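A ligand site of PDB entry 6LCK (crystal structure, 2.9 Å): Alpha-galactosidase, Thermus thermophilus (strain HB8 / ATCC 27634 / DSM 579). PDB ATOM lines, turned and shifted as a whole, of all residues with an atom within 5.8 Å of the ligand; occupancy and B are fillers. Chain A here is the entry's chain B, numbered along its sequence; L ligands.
An oxygen (O4) of the ligand lies within hydrogen-bond range of the side-chain carboxylate of Asp 358 (2.5 Å). The guanidinium group of Arg 368 sits at hydrogen-bond distance from an oxygen (O1) of the ligand (2.5 Å). An oxygen (O2) of the ligand sits at hydrogen-bond distance from the side-chain amide nitrogen of Gln 76 (2.6 Å). O6 of the ligand sits at hydrogen-bond distance from OD1 of Asp 196, at 2.7 Å. NZ of Lys 302 sits at hydrogen-bond distance from O5 of the ligand (2.8 Å). An oxygen (O5) of the ligand sits at hydrogen-bond distance from the side-chain hydroxyl of Tyr 167. An oxygen (O8) of the ligand sits at hydrogen-bond distance from the side-chain carboxylate of Asp 197. O6 of the ligand sits close to OD2 of Asp 304 (3.4 Å). An oxygen (O4) of the ligand is in hydrogen-bond range of the guanidinium group (NH1) of Arg 354 (3.0 Å). The side-chain sulfur of Cys 339 sits at hydrogen-bond distance from an oxygen (O4) of the ligand. The indole nitrogen (NE1) of Trp 233 lies within hydrogen-bond range of an oxygen (O6) of the ligand (3.3 Å). The indole nitrogen of Trp 53 is in hydrogen-bond range of an oxygen (O4) of the ligand (3.4 Å).
The side-chain carboxylate of Asp 358 lies within salt-bridge range of the guanidinium group of Arg 354 (2.9 Å). NE of Arg 368 lies within salt-bridge range of OD2 of Asp 374, 2.8 Å away. NZ of Lys 302 lies within salt-bridge range of OD2 of Asp 196. The side-chain hydroxyl of Tyr 167 sits at hydrogen-bond distance from the side-chain carboxylate of Asp 402, at 2.4 Å. NE1 of Trp 268 is in hydrogen-bond range of OD2 of Asp 197 (2.8 Å). The guanidinium group (NH1) of Arg 354 lies within hydrogen-bond range of the side-chain sulfur (SG) of Cys 339, at 3.4 Å. N of Phe 305 lies within hydrogen-bond range of O of Cys 339. The side-chain hydroxyl (OG1) of Thr 376 is in hydrogen-bond range of the side-chain carboxylate (OD1) of Asp 374 (2.6 Å).
Trp 166 touches the ligand. CZ2 of Trp 268 touches O8 of the ligand, at 3.7 Å. CE1 of Phe 305 touches O7 of the ligand, 3.6 Å away. O of Thr 376 touches O1 of the ligand, 3.6 Å away. Gly 377 touches the ligand (CA to O1, 3.6 Å). CD of Pro 378 touches O1 of the ligand (3.5 Å). Hydrophobic or aromatic side chains within 4 Å of the ligand: Trp 53, Trp 166, Tyr 167, Trp 233, Trp 268, Phe 305 and Pro 378. The nearest printed residue that does not touch the ligand is Asn 267 (4.03 Å).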
ATOM      1  N   TRP A  53       2.139  13.961  10.307  1.00  0.00           N
ATOM      2  CA  TRP A  53       1.799  12.544  10.255  1.00  0.00           C
ATOM      3  C   TRP A  53       0.311  12.283  10.415  1.00  0.00           C
ATOM      4  O   TRP A  53      -0.109  11.137  10.246  1.00  0.00           O
ATOM      5  CB  TRP A  53       2.606  11.789  11.314  1.00  0.00           C
ATOM      6  CG  TRP A  53       4.074  12.175  11.274  1.00  0.00           C
ATOM      7  CD1 TRP A  53       4.829  12.449  10.154  1.00  0.00           C
ATOM      8  CD2 TRP A  53       4.955  12.358  12.390  1.00  0.00           C
ATOM      9  NE1 TRP A  53       6.107  12.771  10.515  1.00  0.00           N
ATOM     10  CE2 TRP A  53       6.213  12.728  11.882  1.00  0.00           C
ATOM     11  CE3 TRP A  53       4.806  12.233  13.769  1.00  0.00           C
ATOM     12  CZ2 TRP A  53       7.311  12.991  12.703  1.00  0.00           C
ATOM     13  CZ3 TRP A  53       5.893  12.489  14.595  1.00  0.00           C
ATOM     14  CH2 TRP A  53       7.123  12.865  14.064  1.00  0.00           C
ATOM     15  N   ARG A  73       0.848   6.588  22.316  1.00  0.00           N
ATOM     16  CA  ARG A  73       1.309   7.109  21.056  1.00  0.00           C
ATOM     17  C   ARG A  73       0.430   8.207  20.485  1.00  0.00           C
ATOM     18  O   ARG A  73       0.781   8.776  19.450  1.00  0.00           O
ATOM     19  CB  ARG A  73       1.426   5.986  20.035  1.00  0.00           C
ATOM     20  CG  ARG A  73       2.815   5.444  19.844  1.00  0.00           C
ATOM     21  CD  ARG A  73       2.752   4.561  18.634  1.00  0.00           C
ATOM     22  NE  ARG A  73       3.925   3.735  18.437  1.00  0.00           N
ATOM     23  CZ  ARG A  73       3.895   2.541  17.856  1.00  0.00           C
ATOM     24  NH1 ARG A  73       2.735   2.040  17.429  1.00  0.00           N
ATOM     25  NH2 ARG A  73       5.023   1.852  17.723  1.00  0.00           N
ATOM     26  N   GLN A  76       1.880  11.854  19.546  1.00  0.00           N
ATOM     27  CA  GLN A  76       2.634  11.968  18.315  1.00  0.00           C
ATOM     28  C   GLN A  76       1.830  11.560  17.084  1.00  0.00           C
ATOM     29  O   GLN A  76       2.385  11.476  15.987  1.00  0.00           O
ATOM     30  CB  GLN A  76       3.928  11.150  18.383  1.00  0.00           C
ATOM     31  CG  GLN A  76       3.765   9.658  18.138  1.00  0.00           C
ATOM     32  CD  GLN A  76       4.799   8.820  18.893  1.00  0.00           C
ATOM     33  OE1 GLN A  76       4.756   8.730  20.121  1.00  0.00           O
ATOM     34  NE2 GLN A  76       5.731   8.210  18.170  1.00  0.00           N
ATOM     35  N   TRP A 166      17.890   8.748   5.987  1.00  0.00           N
ATOM     36  CA  TRP A 166      17.054   8.061   6.965  1.00  0.00           C
ATOM     37  C   TRP A 166      16.512   6.751   6.450  1.00  0.00           C
ATOM     38  O   TRP A 166      16.558   5.733   7.156  1.00  0.00           O
ATOM     39  CB  TRP A 166      15.885   8.945   7.390  1.00  0.00           C
ATOM     40  CG  TRP A 166      14.958   8.226   8.325  1.00  0.00           C
ATOM     41  CD1 TRP A 166      13.696   7.795   8.057  1.00  0.00           C
ATOM     42  CD2 TRP A 166      15.240   7.858   9.684  1.00  0.00           C
ATOM     43  NE1 TRP A 166      13.160   7.185   9.176  1.00  0.00           N
ATOM     44  CE2 TRP A 166      14.089   7.216  10.186  1.00  0.00           C
ATOM     45  CE3 TRP A 166      16.336   8.020  10.531  1.00  0.00           C
ATOM     46  CZ2 TRP A 166      14.020   6.743  11.484  1.00  0.00           C
ATOM     47  CZ3 TRP A 166      16.261   7.525  11.800  1.00  0.00           C
ATOM     48  CH2 TRP A 166      15.115   6.898  12.267  1.00  0.00           C
ATOM     49  N   TYR A 167      15.948   6.757   5.235  1.00  0.00           N
ATOM     50  CA  TYR A 167      15.142   5.644   4.760  1.00  0.00           C
ATOM     51  C   TYR A 167      15.987   4.574   4.099  1.00  0.00           C
ATOM     52  O   TYR A 167      15.563   3.902   3.160  1.00  0.00           O
ATOM     53  CB  TYR A 167      14.068   6.155   3.805  1.00  0.00           C
ATOM     54  CG  TYR A 167      13.083   7.075   4.454  1.00  0.00           C
ATOM     55  CD1 TYR A 167      11.978   6.576   5.126  1.00  0.00           C
ATOM     56  CD2 TYR A 167      13.251   8.458   4.416  1.00  0.00           C
ATOM     57  CE1 TYR A 167      11.045   7.443   5.717  1.00  0.00           C
ATOM     58  CE2 TYR A 167      12.326   9.322   5.004  1.00  0.00           C
ATOM     59  CZ  TYR A 167      11.237   8.794   5.650  1.00  0.00           C
ATOM     60  OH  TYR A 167      10.320   9.614   6.237  1.00  0.00           O
ATOM     61  N   THR A 171      18.911   4.936  12.183  1.00  0.00           N
ATOM     62  CA  THR A 171      19.807   5.529  13.168  1.00  0.00           C
ATOM     63  C   THR A 171      21.224   4.998  13.052  1.00  0.00           C
ATOM     64  O   THR A 171      22.143   5.587  13.629  1.00  0.00           O
ATOM     65  CB  THR A 171      19.318   5.289  14.599  1.00  0.00           C
ATOM     66  OG1 THR A 171      19.220   3.889  14.836  1.00  0.00           O
ATOM     67  CG2 THR A 171      17.978   5.933  14.803  1.00  0.00           C
ATOM     68  N   ASP A 196      20.340  12.532   8.569  1.00  0.00           N
ATOM     69  CA  ASP A 196      19.118  12.459   9.363  1.00  0.00           C
ATOM     70  C   ASP A 196      19.413  11.992  10.795  1.00  0.00           C
ATOM     71  O   ASP A 196      20.531  12.157  11.296  1.00  0.00           O
ATOM     72  CB  ASP A 196      18.087  11.583   8.662  1.00  0.00           C
ATOM     73  CG  ASP A 196      16.664  12.068   8.908  1.00  0.00           C
ATOM     74  OD1 ASP A 196      16.021  11.563   9.859  1.00  0.00           O
ATOM     75  OD2 ASP A 196      16.222  13.000   8.187  1.00  0.00           O
ATOM     76  N   ASP A 197      18.397  11.456  11.470  1.00  0.00           N
ATOM     77  CA  ASP A 197      18.550  10.959  12.833  1.00  0.00           C
ATOM     78  C   ASP A 197      19.688   9.944  12.895  1.00  0.00           C
ATOM     79  O   ASP A 197      19.780   9.058  12.034  1.00  0.00           O
ATOM     80  CB  ASP A 197      17.238  10.327  13.303  1.00  0.00           C
ATOM     81  CG  ASP A 197      17.231   9.869  14.780  1.00  0.00           C
ATOM     82  OD1 ASP A 197      18.189  10.152  15.521  1.00  0.00           O
ATOM     83  OD2 ASP A 197      16.235   9.222  15.188  1.00  0.00           O
ATOM     84  N   TRP A 233      19.552  17.185  10.732  1.00  0.00           N
ATOM     85  CA  TRP A 233      18.279  16.865  11.349  1.00  0.00           C
ATOM     86  C   TRP A 233      18.318  17.161  12.846  1.00  0.00           C
ATOM     87  O   TRP A 233      19.285  16.817  13.536  1.00  0.00           O
ATOM     88  CB  TRP A 233      17.962  15.388  11.123  1.00  0.00           C
ATOM     89  CG  TRP A 233      16.745  14.833  11.844  1.00  0.00           C
ATOM     90  CD1 TRP A 233      15.465  14.736  11.352  1.00  0.00           C
ATOM     91  CD2 TRP A 233      16.700  14.273  13.168  1.00  0.00           C
ATOM     92  NE1 TRP A 233      14.640  14.166  12.280  1.00  0.00           N
ATOM     93  CE2 TRP A 233      15.367  13.871  13.407  1.00  0.00           C
ATOM     94  CE3 TRP A 233      17.655  14.086  14.175  1.00  0.00           C
ATOM     95  CZ2 TRP A 233      14.962  13.306  14.608  1.00  0.00           C
ATOM     96  CZ3 TRP A 233      17.244  13.502  15.379  1.00  0.00           C
ATOM     97  CH2 TRP A 233      15.913  13.138  15.584  1.00  0.00           C
ATOM     98  N   PHE A 266       5.895   8.173  22.319  1.00  0.00           N
ATOM     99  CA  PHE A 266       6.685   6.986  22.637  1.00  0.00           C
ATOM    100  C   PHE A 266       7.459   6.629  21.369  1.00  0.00           C
ATOM    101  O   PHE A 266       6.852   6.273  20.356  1.00  0.00           O
ATOM    102  CB  PHE A 266       5.802   5.818  23.073  1.00  0.00           C
ATOM    103  CG  PHE A 266       6.564   4.677  23.704  1.00  0.00           C
ATOM    104  CD1 PHE A 266       7.235   3.746  22.907  1.00  0.00           C
ATOM    105  CD2 PHE A 266       6.603   4.518  25.086  1.00  0.00           C
ATOM    106  CE1 PHE A 266       7.937   2.678  23.482  1.00  0.00           C
ATOM    107  CE2 PHE A 266       7.312   3.451  25.680  1.00  0.00           C
ATOM    108  CZ  PHE A 266       7.973   2.533  24.875  1.00  0.00           C
ATOM    109  N   ASN A 267       8.769   6.738  21.430  1.00  0.00           N
ATOM    110  CA  ASN A 267       9.570   6.446  20.246  1.00  0.00           C
ATOM    111  C   ASN A 267      10.965   6.122  20.743  1.00  0.00           C
ATOM    112  O   ASN A 267      11.305   6.394  21.898  1.00  0.00           O
ATOM    113  CB  ASN A 267       9.541   7.614  19.267  1.00  0.00           C
ATOM    114  CG  ASN A 267      10.104   7.243  17.902  1.00  0.00           C
ATOM    115  OD1 ASN A 267       9.865   6.141  17.398  1.00  0.00           O
ATOM    116  ND2 ASN A 267      10.797   8.192  17.270  1.00  0.00           N
ATOM    117  N   TRP A 268      11.772   5.509  19.871  1.00  0.00           N
ATOM    118  CA  TRP A 268      13.057   4.953  20.262  1.00  0.00           C
ATOM    119  C   TRP A 268      12.931   4.095  21.537  1.00  0.00           C
ATOM    120  O   TRP A 268      13.798   4.107  22.410  1.00  0.00           O
ATOM    121  CB  TRP A 268      14.098   6.048  20.460  1.00  0.00           C
ATOM    122  CG  TRP A 268      14.312   6.934  19.293  1.00  0.00           C
ATOM    123  CD1 TRP A 268      15.139   6.711  18.225  1.00  0.00           C
ATOM    124  CD2 TRP A 268      13.720   8.223  19.076  1.00  0.00           C
ATOM    125  NE1 TRP A 268      15.100   7.771  17.358  1.00  0.00           N
ATOM    126  CE2 TRP A 268      14.239   8.720  17.849  1.00  0.00           C
ATOM    127  CE3 TRP A 268      12.820   9.001  19.795  1.00  0.00           C
ATOM    128  CZ2 TRP A 268      13.864   9.961  17.330  1.00  0.00           C
ATOM    129  CZ3 TRP A 268      12.449  10.242  19.285  1.00  0.00           C
ATOM    130  CH2 TRP A 268      12.968  10.708  18.059  1.00  0.00           C
ATOM    131  N   LYS A 302      16.430  19.962   8.857  1.00  0.00           N
ATOM    132  CA  LYS A 302      15.195  19.184   8.999  1.00  0.00           C
ATOM    133  C   LYS A 302      14.781  19.231  10.472  1.00  0.00           C
ATOM    134  O   LYS A 302      15.384  18.562  11.323  1.00  0.00           O
ATOM    135  CB  LYS A 302      15.369  17.744   8.515  1.00  0.00           C
ATOM    136  CG  LYS A 302      14.120  16.855   8.655  1.00  0.00           C
ATOM    137  CD  LYS A 302      14.293  15.530   7.915  1.00  0.00           C
ATOM    138  CE  LYS A 302      13.058  14.650   7.987  1.00  0.00           C
ATOM    139  NZ  LYS A 302      13.252  13.373   7.261  1.00  0.00           N
ATOM    140  N   ASP A 304      12.348  18.375  13.234  1.00  0.00           N
ATOM    141  CA  ASP A 304      11.430  17.264  13.365  1.00  0.00           C
ATOM    142  C   ASP A 304      10.747  17.261  14.738  1.00  0.00           C
ATOM    143  O   ASP A 304      11.181  17.912  15.694  1.00  0.00           O
ATOM    144  CB  ASP A 304      12.168  15.943  13.145  1.00  0.00           C
ATOM    145  CG  ASP A 304      11.240  14.825  12.773  1.00  0.00           C
ATOM    146  OD1 ASP A 304      10.032  15.071  12.596  1.00  0.00           O
ATOM    147  OD2 ASP A 304      11.740  13.684  12.690  1.00  0.00           O
ATOM    148  N   PHE A 305       9.651  16.486  14.792  1.00  0.00           N
ATOM    149  CA  PHE A 305       8.815  16.337  15.977  1.00  0.00           C
ATOM    150  C   PHE A 305       8.297  17.681  16.482  1.00  0.00           C
ATOM    151  O   PHE A 305       8.075  17.880  17.677  1.00  0.00           O
ATOM    152  CB  PHE A 305       9.562  15.571  17.067  1.00  0.00           C
ATOM    153  CG  PHE A 305       9.760  14.102  16.755  1.00  0.00           C
ATOM    154  CD1 PHE A 305      10.751  13.687  15.881  1.00  0.00           C
ATOM    155  CD2 PHE A 305       8.916  13.136  17.311  1.00  0.00           C
ATOM    156  CE1 PHE A 305      10.931  12.342  15.592  1.00  0.00           C
ATOM    157  CE2 PHE A 305       9.092  11.791  17.013  1.00  0.00           C
ATOM    158  CZ  PHE A 305      10.099  11.395  16.165  1.00  0.00           C
ATOM    159  N   CYS A 339       8.851  18.969   9.926  1.00  0.00           N
ATOM    160  CA  CYS A 339       8.423  17.586   9.945  1.00  0.00           C
ATOM    161  C   CYS A 339       7.713  17.313  11.270  1.00  0.00           C
ATOM    162  O   CYS A 339       8.078  17.878  12.305  1.00  0.00           O
ATOM    163  CB  CYS A 339       9.638  16.654   9.747  1.00  0.00           C
ATOM    164  SG  CYS A 339       9.207  14.922   9.565  1.00  0.00           S
ATOM    165  N   GLY A 340       6.671  16.490  11.234  1.00  0.00           N
ATOM    166  CA  GLY A 340       5.855  16.317  12.435  1.00  0.00           C
ATOM    167  C   GLY A 340       5.293  17.622  12.945  1.00  0.00           C
ATOM    168  O   GLY A 340       5.101  17.803  14.151  1.00  0.00           O
ATOM    169  N   ARG A 354       6.600  18.479   5.509  1.00  0.00           N
ATOM    170  CA  ARG A 354       6.083  17.117   5.399  1.00  0.00           C
ATOM    171  C   ARG A 354       4.561  17.143   5.604  1.00  0.00           C
ATOM    172  O   ARG A 354       4.074  17.709   6.593  1.00  0.00           O
ATOM    173  CB  ARG A 354       6.775  16.222   6.415  1.00  0.00           C
ATOM    174  CG  ARG A 354       8.152  15.798   5.962  1.00  0.00           C
ATOM    175  CD  ARG A 354       8.037  14.652   4.965  1.00  0.00           C
ATOM    176  NE  ARG A 354       7.259  13.577   5.565  1.00  0.00           N
ATOM    177  CZ  ARG A 354       7.740  12.763   6.491  1.00  0.00           C
ATOM    178  NH1 ARG A 354       9.000  12.896   6.883  1.00  0.00           N
ATOM    179  NH2 ARG A 354       6.976  11.824   7.030  1.00  0.00           N
ATOM    180  N   ASP A 358       5.469   8.993   7.399  1.00  0.00           N
ATOM    181  CA  ASP A 358       6.673   8.415   6.806  1.00  0.00           C
ATOM    182  C   ASP A 358       6.327   7.438   5.702  1.00  0.00           C
ATOM    183  O   ASP A 358       5.544   6.495   5.910  1.00  0.00           O
ATOM    184  CB  ASP A 358       7.474   7.649   7.857  1.00  0.00           C
ATOM    185  CG  ASP A 358       8.216   8.526   8.822  1.00  0.00           C
ATOM    186  OD1 ASP A 358       7.957   9.760   8.876  1.00  0.00           O
ATOM    187  OD2 ASP A 358       9.068   7.945   9.536  1.00  0.00           O
ATOM    188  N   ARG A 368      -0.395  -2.223  12.640  1.00  0.00           N
ATOM    189  CA  ARG A 368      -0.520  -0.876  13.163  1.00  0.00           C
ATOM    190  C   ARG A 368      -1.672  -0.101  12.554  1.00  0.00           C
ATOM    191  O   ARG A 368      -2.386   0.602  13.277  1.00  0.00           O
ATOM    192  CB  ARG A 368       0.773  -0.114  12.949  1.00  0.00           C
ATOM    193  CG  ARG A 368       0.778   1.186  13.652  1.00  0.00           C
ATOM    194  CD  ARG A 368       2.157   1.774  13.677  1.00  0.00           C
ATOM    195  NE  ARG A 368       2.058   3.140  14.159  1.00  0.00           N
ATOM    196  CZ  ARG A 368       3.095   3.911  14.440  1.00  0.00           C
ATOM    197  NH1 ARG A 368       4.344   3.477  14.282  1.00  0.00           N
ATOM    198  NH2 ARG A 368       2.854   5.134  14.868  1.00  0.00           N
ATOM    199  N   ASP A 374      -4.287   3.104  13.702  1.00  0.00           N
ATOM    200  CA  ASP A 374      -3.284   4.166  13.713  1.00  0.00           C
ATOM    201  C   ASP A 374      -2.807   4.400  12.286  1.00  0.00           C
ATOM    202  O   ASP A 374      -1.818   3.796  11.839  1.00  0.00           O
ATOM    203  CB  ASP A 374      -2.120   3.771  14.625  1.00  0.00           C
ATOM    204  CG  ASP A 374      -1.020   4.834  14.698  1.00  0.00           C
ATOM    205  OD1 ASP A 374      -1.177   5.908  14.101  1.00  0.00           O
ATOM    206  OD2 ASP A 374       0.008   4.564  15.367  1.00  0.00           O
ATOM    207  N   THR A 376      -1.173   6.840  11.169  1.00  0.00           N
ATOM    208  CA  THR A 376      -0.056   7.772  11.157  1.00  0.00           C
ATOM    209  C   THR A 376       1.289   7.063  11.205  1.00  0.00           C
ATOM    210  O   THR A 376       2.328   7.729  11.151  1.00  0.00           O
ATOM    211  CB  THR A 376      -0.177   8.777  12.319  1.00  0.00           C
ATOM    212  OG1 THR A 376       0.120   8.129  13.565  1.00  0.00           O
ATOM    213  CG2 THR A 376      -1.587   9.373  12.389  1.00  0.00           C
ATOM    214  N   GLY A 377       1.275   5.726  11.297  1.00  0.00           N
ATOM    215  CA  GLY A 377       2.494   4.948  11.263  1.00  0.00           C
ATOM    216  C   GLY A 377       3.178   5.004   9.909  1.00  0.00           C
ATOM    217  O   GLY A 377       2.577   5.380   8.886  1.00  0.00           O
ATOM    218  N   PRO A 378       4.465   4.659   9.883  1.00  0.00           N
ATOM    219  CA  PRO A 378       5.174   4.613   8.608  1.00  0.00           C
ATOM    220  C   PRO A 378       4.520   3.628   7.648  1.00  0.00           C
ATOM    221  O   PRO A 378       3.983   2.584   8.042  1.00  0.00           O
ATOM    222  CB  PRO A 378       6.583   4.167   8.998  1.00  0.00           C
ATOM    223  CG  PRO A 378       6.702   4.596  10.401  1.00  0.00           C
ATOM    224  CD  PRO A 378       5.356   4.476  11.027  1.00  0.00           C
ATOM    225  N   ASP A 402       7.690  13.148   1.073  1.00  0.00           N
ATOM    226  CA  ASP A 402       8.694  12.256   1.650  1.00  0.00           C
ATOM    227  C   ASP A 402       9.437  11.518   0.540  1.00  0.00           C
ATOM    228  O   ASP A 402       9.137  11.701  -0.651  1.00  0.00           O
ATOM    229  CB  ASP A 402       8.075  11.277   2.648  1.00  0.00           C
ATOM    230  CG  ASP A 402       9.019  10.864   3.748  1.00  0.00           C
ATOM    231  OD1 ASP A 402      10.219  11.235   3.712  1.00  0.00           O
ATOM    232  OD2 ASP A 402       8.550  10.134   4.648  1.00  0.00           O
HETATM  233  C1  LIG L   1      13.937  10.223  12.318  1.00  0.00           C
HETATM  234  C2  LIG L   1      12.616  10.112  11.608  1.00  0.00           C
HETATM  235  C3  LIG L   1      12.757  10.654  10.189  1.00  0.00           C
HETATM  236  C4  LIG L   1      11.416  10.729   9.502  1.00  0.00           C
HETATM  237  C5  LIG L   1      10.442  11.537  10.371  1.00  0.00           C
HETATM  238  C6  LIG L   1      10.202  10.836  11.711  1.00  0.00           C
HETATM  239  O1  LIG L   1       4.553   6.611  13.743  1.00  0.00           O
HETATM  240  N1  LIG L   1       5.461   7.507  14.485  1.00  0.00           N
HETATM  241  O2  LIG L   1       5.192   7.858  15.618  1.00  0.00           O
HETATM  242  C7  LIG L   1       6.617   8.001  13.807  1.00  0.00           C
HETATM  243  C8  LIG L   1       6.392   8.521  12.541  1.00  0.00           C
HETATM  244  C9  LIG L   1       7.457   9.015  11.819  1.00  0.00           C
HETATM  245  C10 LIG L   1       8.770   9.003  12.356  1.00  0.00           C
HETATM  246  C11 LIG L   1       8.996   8.433  13.644  1.00  0.00           C
HETATM  247  C12 LIG L   1       7.928   7.938  14.356  1.00  0.00           C
HETATM  248  O3  LIG L   1       9.851   9.534  11.544  1.00  0.00           O
HETATM  249  O4  LIG L   1       9.279  11.764   9.632  1.00  0.00           O
HETATM  250  O5  LIG L   1      11.537  11.310   8.184  1.00  0.00           O
HETATM  251  O6  LIG L   1      13.338  11.956  10.217  1.00  0.00           O
HETATM  252  O7  LIG L   1      11.524  10.802  12.435  1.00  0.00           O
HETATM  253  O8  LIG L   1      13.814   9.649  13.690  1.00  0.00           O
